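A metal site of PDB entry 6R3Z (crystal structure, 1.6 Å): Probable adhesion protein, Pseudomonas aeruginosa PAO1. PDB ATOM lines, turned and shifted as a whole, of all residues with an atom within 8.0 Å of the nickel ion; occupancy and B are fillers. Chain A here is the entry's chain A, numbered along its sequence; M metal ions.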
ATOM      1  N   LEU A  13     -10.428  27.329 -17.894  1.00  0.00           N
ATOM      2  CA  LEU A  13      -9.923  28.321 -16.942  1.00  0.00           C
ATOM      3  C   LEU A  13      -9.163  29.419 -17.695  1.00  0.00           C
ATOM      4  O   LEU A  13      -8.600  29.155 -18.765  1.00  0.00           O
ATOM      5  CB  LEU A  13      -8.999  27.654 -15.898  1.00  0.00           C
ATOM      6  CG  LEU A  13      -9.557  26.401 -15.183  1.00  0.00           C
ATOM      7  CD1 LEU A  13      -8.455  25.647 -14.471  1.00  0.00           C
ATOM      8  CD2 LEU A  13     -10.688  26.751 -14.193  1.00  0.00           C
ATOM      9  N   ASN A  39     -16.745  32.089 -10.379  1.00  0.00           N
ATOM     10  CA  ASN A  39     -15.653  31.432  -9.650  1.00  0.00           C
ATOM     11  C   ASN A  39     -15.645  29.977 -10.117  1.00  0.00           C
ATOM     12  O   ASN A  39     -16.646  29.272  -9.944  1.00  0.00           O
ATOM     13  CB  ASN A  39     -15.866  31.532  -8.144  1.00  0.00           C
ATOM     14  CG  ASN A  39     -14.758  30.957  -7.282  1.00  0.00           C
ATOM     15  OD1 ASN A  39     -13.811  30.320  -7.771  1.00  0.00           O
ATOM     16  ND2 ASN A  39     -14.853  31.181  -5.981  1.00  0.00           N
ATOM     17  N   PRO A  40     -14.563  29.523 -10.774  1.00  0.00           N
ATOM     18  CA  PRO A  40     -14.528  28.126 -11.246  1.00  0.00           C
ATOM     19  C   PRO A  40     -14.608  27.082 -10.123  1.00  0.00           C
ATOM     20  O   PRO A  40     -14.990  25.940 -10.380  1.00  0.00           O
ATOM     21  CB  PRO A  40     -13.228  28.046 -12.055  1.00  0.00           C
ATOM     22  CG  PRO A  40     -12.349  29.099 -11.438  1.00  0.00           C
ATOM     23  CD  PRO A  40     -13.286  30.223 -11.053  1.00  0.00           C
ATOM     24  N   HIS A  41     -14.264  27.484  -8.870  1.00  0.00           N
ATOM     25  CA  HIS A  41     -14.348  26.609  -7.695  1.00  0.00           C
ATOM     26  C   HIS A  41     -15.794  26.316  -7.299  1.00  0.00           C
ATOM     27  O   HIS A  41     -16.063  25.280  -6.705  1.00  0.00           O
ATOM     28  CB  HIS A  41     -13.623  27.219  -6.504  1.00  0.00           C
ATOM     29  CG  HIS A  41     -12.165  27.453  -6.747  1.00  0.00           C
ATOM     30  ND1 HIS A  41     -11.696  28.660  -7.224  1.00  0.00           N
ATOM     31  CD2 HIS A  41     -11.125  26.588  -6.669  1.00  0.00           C
ATOM     32  CE1 HIS A  41     -10.386  28.514  -7.377  1.00  0.00           C
ATOM     33  NE2 HIS A  41     -10.005  27.280  -7.053  1.00  0.00           N
ATOM     34  N   GLY A  65      -7.548  17.980 -11.806  1.00  0.00           N
ATOM     35  CA  GLY A  65      -8.318  18.342 -10.623  1.00  0.00           C
ATOM     36  C   GLY A  65      -8.907  19.745 -10.604  1.00  0.00           C
ATOM     37  O   GLY A  65      -9.673  20.060  -9.685  1.00  0.00           O
ATOM     38  N   HIS A  66      -8.544  20.608 -11.585  1.00  0.00           N
ATOM     39  CA  HIS A  66      -9.103  21.971 -11.560  1.00  0.00           C
ATOM     40  C   HIS A  66     -10.252  22.205 -12.552  1.00  0.00           C
ATOM     41  O   HIS A  66     -10.775  23.319 -12.603  1.00  0.00           O
ATOM     42  CB  HIS A  66      -8.038  23.072 -11.711  1.00  0.00           C
ATOM     43  CG  HIS A  66      -8.277  24.205 -10.742  1.00  0.00           C
ATOM     44  ND1 HIS A  66      -9.472  24.898 -10.743  1.00  0.00           N
ATOM     45  CD2 HIS A  66      -7.522  24.638  -9.705  1.00  0.00           C
ATOM     46  CE1 HIS A  66      -9.384  25.766  -9.742  1.00  0.00           C
ATOM     47  NE2 HIS A  66      -8.238  25.647  -9.088  1.00  0.00           N
ATOM     48  N   ASN A 109      -1.714  18.305  -6.443  1.00  0.00           N
ATOM     49  CA  ASN A 109      -2.051  19.718  -6.550  1.00  0.00           C
ATOM     50  C   ASN A 109      -2.393  20.032  -8.035  1.00  0.00           C
ATOM     51  O   ASN A 109      -1.545  19.900  -8.910  1.00  0.00           O
ATOM     52  CB  ASN A 109      -0.919  20.622  -6.030  1.00  0.00           C
ATOM     53  CG  ASN A 109      -1.365  22.067  -5.855  1.00  0.00           C
ATOM     54  OD1 ASN A 109      -2.104  22.625  -6.691  1.00  0.00           O
ATOM     55  ND2 ASN A 109      -0.921  22.711  -4.784  1.00  0.00           N
ATOM     56  N   PRO A 110      -3.634  20.472  -8.324  1.00  0.00           N
ATOM     57  CA  PRO A 110      -4.010  20.709  -9.735  1.00  0.00           C
ATOM     58  C   PRO A 110      -3.614  22.070 -10.324  1.00  0.00           C
ATOM     59  O   PRO A 110      -3.915  22.322 -11.489  1.00  0.00           O
ATOM     60  CB  PRO A 110      -5.531  20.548  -9.701  1.00  0.00           C
ATOM     61  CG  PRO A 110      -5.922  21.048  -8.343  1.00  0.00           C
ATOM     62  CD  PRO A 110      -4.782  20.697  -7.411  1.00  0.00           C
ATOM     63  N   HIS A 111      -2.989  22.968  -9.523  1.00  0.00           N
ATOM     64  CA  HIS A 111      -2.630  24.338  -9.946  1.00  0.00           C
ATOM     65  C   HIS A 111      -1.333  24.433 -10.755  1.00  0.00           C
ATOM     66  O   HIS A 111      -0.515  25.334 -10.525  1.00  0.00           O
ATOM     67  CB  HIS A 111      -2.593  25.285  -8.735  1.00  0.00           C
ATOM     68  CG  HIS A 111      -3.882  25.340  -7.990  1.00  0.00           C
ATOM     69  ND1 HIS A 111      -4.146  24.459  -6.948  1.00  0.00           N
ATOM     70  CD2 HIS A 111      -4.926  26.194  -8.120  1.00  0.00           C
ATOM     71  CE1 HIS A 111      -5.351  24.792  -6.489  1.00  0.00           C
ATOM     72  NE2 HIS A 111      -5.868  25.819  -7.179  1.00  0.00           N
ATOM     73  N   PHE A 113      -0.909  25.366 -13.732  1.00  0.00           N
ATOM     74  CA  PHE A 113      -0.886  26.616 -14.523  1.00  0.00           C
ATOM     75  C   PHE A 113      -0.219  27.779 -13.770  1.00  0.00           C
ATOM     76  O   PHE A 113       0.145  28.756 -14.402  1.00  0.00           O
ATOM     77  CB  PHE A 113      -2.298  27.013 -15.002  1.00  0.00           C
ATOM     78  CG  PHE A 113      -3.356  26.909 -13.937  1.00  0.00           C
ATOM     79  CD1 PHE A 113      -3.654  27.999 -13.124  1.00  0.00           C
ATOM     80  CD2 PHE A 113      -4.074  25.724 -13.755  1.00  0.00           C
ATOM     81  CE1 PHE A 113      -4.650  27.919 -12.144  1.00  0.00           C
ATOM     82  CE2 PHE A 113      -5.060  25.627 -12.759  1.00  0.00           C
ATOM     83  CZ  PHE A 113      -5.328  26.728 -11.952  1.00  0.00           C
ATOM     84  N   LEU A 114      -0.050  27.678 -12.441  1.00  0.00           N
ATOM     85  CA  LEU A 114       0.626  28.744 -11.706  1.00  0.00           C
ATOM     86  C   LEU A 114       2.107  28.424 -11.518  1.00  0.00           C
ATOM     87  O   LEU A 114       2.634  28.437 -10.422  1.00  0.00           O
ATOM     88  CB  LEU A 114      -0.094  29.113 -10.393  1.00  0.00           C
ATOM     89  CG  LEU A 114      -1.554  29.581 -10.552  1.00  0.00           C
ATOM     90  CD1 LEU A 114      -2.274  29.609  -9.221  1.00  0.00           C
ATOM     91  CD2 LEU A 114      -1.646  30.907 -11.259  1.00  0.00           C
ATOM     92  N   HIS A 177      -5.251  29.677  -0.088  1.00  0.00           N
ATOM     93  CA  HIS A 177      -5.638  28.703  -1.111  1.00  0.00           C
ATOM     94  C   HIS A 177      -4.390  27.874  -1.461  1.00  0.00           C
ATOM     95  O   HIS A 177      -3.298  28.428  -1.495  1.00  0.00           O
ATOM     96  CB  HIS A 177      -6.182  29.431  -2.349  1.00  0.00           C
ATOM     97  CG  HIS A 177      -6.934  28.578  -3.318  1.00  0.00           C
ATOM     98  ND1 HIS A 177      -8.299  28.327  -3.155  1.00  0.00           N
ATOM     99  CD2 HIS A 177      -6.540  28.030  -4.489  1.00  0.00           C
ATOM    100  CE1 HIS A 177      -8.658  27.610  -4.217  1.00  0.00           C
ATOM    101  NE2 HIS A 177      -7.643  27.432  -5.059  1.00  0.00           N
ATOM    102  N   GLY A 178      -4.561  26.568  -1.695  1.00  0.00           N
ATOM    103  CA  GLY A 178      -3.420  25.699  -2.016  1.00  0.00           C
ATOM    104  C   GLY A 178      -2.966  25.804  -3.473  1.00  0.00           C
ATOM    105  O   GLY A 178      -2.702  24.787  -4.116  1.00  0.00           O
ATOM    106  N   ALA A 179      -2.866  27.036  -4.005  1.00  0.00           N
ATOM    107  CA  ALA A 179      -2.580  27.297  -5.416  1.00  0.00           C
ATOM    108  C   ALA A 179      -1.128  27.549  -5.784  1.00  0.00           C
ATOM    109  O   ALA A 179      -0.826  27.598  -6.983  1.00  0.00           O
ATOM    110  CB  ALA A 179      -3.401  28.508  -5.859  1.00  0.00           C
ATOM    111  N   TYR A 180      -0.240  27.811  -4.796  1.00  0.00           N
ATOM    112  CA  TYR A 180       1.095  28.352  -5.083  1.00  0.00           C
ATOM    113  C   TYR A 180       2.299  27.445  -4.842  1.00  0.00           C
ATOM    114  O   TYR A 180       3.435  27.925  -4.919  1.00  0.00           O
ATOM    115  CB  TYR A 180       1.237  29.673  -4.308  1.00  0.00           C
ATOM    116  CG  TYR A 180       0.092  30.602  -4.620  1.00  0.00           C
ATOM    117  CD1 TYR A 180      -0.069  31.135  -5.896  1.00  0.00           C
ATOM    118  CD2 TYR A 180      -0.960  30.771  -3.722  1.00  0.00           C
ATOM    119  CE1 TYR A 180      -1.172  31.929  -6.234  1.00  0.00           C
ATOM    120  CE2 TYR A 180      -2.073  31.559  -4.041  1.00  0.00           C
ATOM    121  CZ  TYR A 180      -2.190  32.103  -5.305  1.00  0.00           C
ATOM    122  OH  TYR A 180      -3.284  32.876  -5.649  1.00  0.00           O
ATOM    123  N   GLU A 196      -6.916  26.780   3.987  1.00  0.00           N
ATOM    124  CA  GLU A 196      -8.084  26.010   3.538  1.00  0.00           C
ATOM    125  C   GLU A 196      -7.818  24.507   3.754  1.00  0.00           C
ATOM    126  O   GLU A 196      -6.792  23.985   3.284  1.00  0.00           O
ATOM    127  CB  GLU A 196      -8.395  26.301   2.074  1.00  0.00           C
ATOM    128  CG  GLU A 196      -9.037  27.659   1.888  1.00  0.00           C
ATOM    129  CD  GLU A 196      -9.509  27.988   0.487  1.00  0.00           C
ATOM    130  OE1 GLU A 196      -9.094  27.294  -0.481  1.00  0.00           O
ATOM    131  OE2 GLU A 196     -10.313  28.925   0.356  1.00  0.00           O
ATOM    132  N   HIS A 199      -9.087  21.927  -1.164  1.00  0.00           N
ATOM    133  CA  HIS A 199      -9.217  22.846  -2.303  1.00  0.00           C
ATOM    134  C   HIS A 199     -10.550  23.607  -2.335  1.00  0.00           C
ATOM    135  O   HIS A 199     -11.615  23.002  -2.539  1.00  0.00           O
ATOM    136  CB  HIS A 199      -8.992  22.107  -3.642  1.00  0.00           C
ATOM    137  CG  HIS A 199      -8.898  23.028  -4.819  1.00  0.00           C
ATOM    138  ND1 HIS A 199      -9.337  22.653  -6.080  1.00  0.00           N
ATOM    139  CD2 HIS A 199      -8.395  24.291  -4.898  1.00  0.00           C
ATOM    140  CE1 HIS A 199      -9.097  23.690  -6.864  1.00  0.00           C
ATOM    141  NE2 HIS A 199      -8.566  24.698  -6.205  1.00  0.00           N
ATOM    142  N   GLY A 200     -10.479  24.918  -2.060  1.00  0.00           N
ATOM    143  CA  GLY A 200     -11.598  25.843  -2.096  1.00  0.00           C
ATOM    144  C   GLY A 200     -12.608  25.707  -0.977  1.00  0.00           C
ATOM    145  O   GLY A 200     -13.703  26.275  -1.069  1.00  0.00           O
ATOM    146  N   GLU A 226      -5.712  35.501  -1.254  1.00  0.00           N
ATOM    147  CA  GLU A 226      -6.299  35.559  -2.595  1.00  0.00           C
ATOM    148  C   GLU A 226      -6.816  36.935  -2.975  1.00  0.00           C
ATOM    149  O   GLU A 226      -7.652  37.496  -2.273  1.00  0.00           O
ATOM    150  CB  GLU A 226      -7.493  34.566  -2.690  1.00  0.00           C
ATOM    151  CG  GLU A 226      -7.097  33.089  -2.638  1.00  0.00           C
ATOM    152  CD  GLU A 226      -6.206  32.733  -3.805  1.00  0.00           C
ATOM    153  OE1 GLU A 226      -6.724  32.619  -4.941  1.00  0.00           O
ATOM    154  OE2 GLU A 226      -4.976  32.655  -3.588  1.00  0.00           O
ATOM    155  N   HIS A 250      -4.964  33.893  -8.551  1.00  0.00           N
ATOM    156  CA  HIS A 250      -5.200  32.527  -9.038  1.00  0.00           C
ATOM    157  C   HIS A 250      -5.445  32.628 -10.583  1.00  0.00           C
ATOM    158  O   HIS A 250      -5.653  31.601 -11.243  1.00  0.00           O
ATOM    159  CB  HIS A 250      -6.494  32.011  -8.352  1.00  0.00           C
ATOM    160  CG  HIS A 250      -6.760  30.526  -8.437  1.00  0.00           C
ATOM    161  ND1 HIS A 250      -7.074  29.911  -9.650  1.00  0.00           N
ATOM    162  CD2 HIS A 250      -6.935  29.632  -7.440  1.00  0.00           C
ATOM    163  CE1 HIS A 250      -7.380  28.655  -9.339  1.00  0.00           C
ATOM    164  NE2 HIS A 250      -7.298  28.434  -8.023  1.00  0.00           N
ATOM    165  N   SER A 252      -8.142  33.926 -12.156  1.00  0.00           N
ATOM    166  CA  SER A 252      -9.473  33.341 -12.301  1.00  0.00           C
ATOM    167  C   SER A 252     -10.590  34.377 -12.272  1.00  0.00           C
ATOM    168  O   SER A 252     -11.749  33.978 -12.306  1.00  0.00           O
ATOM    169  CB  SER A 252      -9.692  32.357 -11.159  1.00  0.00           C
ATOM    170  OG  SER A 252      -9.839  33.064  -9.933  1.00  0.00           O
HETATM  171 NI    NI M   1      -7.935  26.574  -7.045  1.00  0.00          NI
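The nickel ion is bound by a ring nitrogen (NE2) of His 199 (2.2 Å), a ring nitrogen (NE2) of His 177 (2.2 Å), a ring nitrogen (NE2) of His 41 (2.2 Å), a ring nitrogen (NE2) of His 250 (2.2 Å), a ring nitrogen (NE2) of His 111 (2.2 Å) and a ring nitrogen (NE2) of His 66 (2.3 Å).
The nickel ion has six donor atoms within binding distance.
Within 4 Å of the nickel ion: His 41, His 66, His 111, His 177, His 199 and His 250.
A ring nitrogen (ND1) of His 177 is in hydrogen-bond range of the side-chain carboxylate of Glu 196.
ND1 of His 41 sits at hydrogen-bond distance from OD1 of Asn 39 (2.7 Å).
The backbone carbonyl oxygen (O) of Gly 178 lies within hydrogen-bond range of a ring nitrogen (ND1) of His 111 (3.2 Å).
A ring nitrogen (ND1) of His 111 lies within hydrogen-bond range of the side-chain amide oxygen (OD1) of Asn 109 (2.8 Å).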
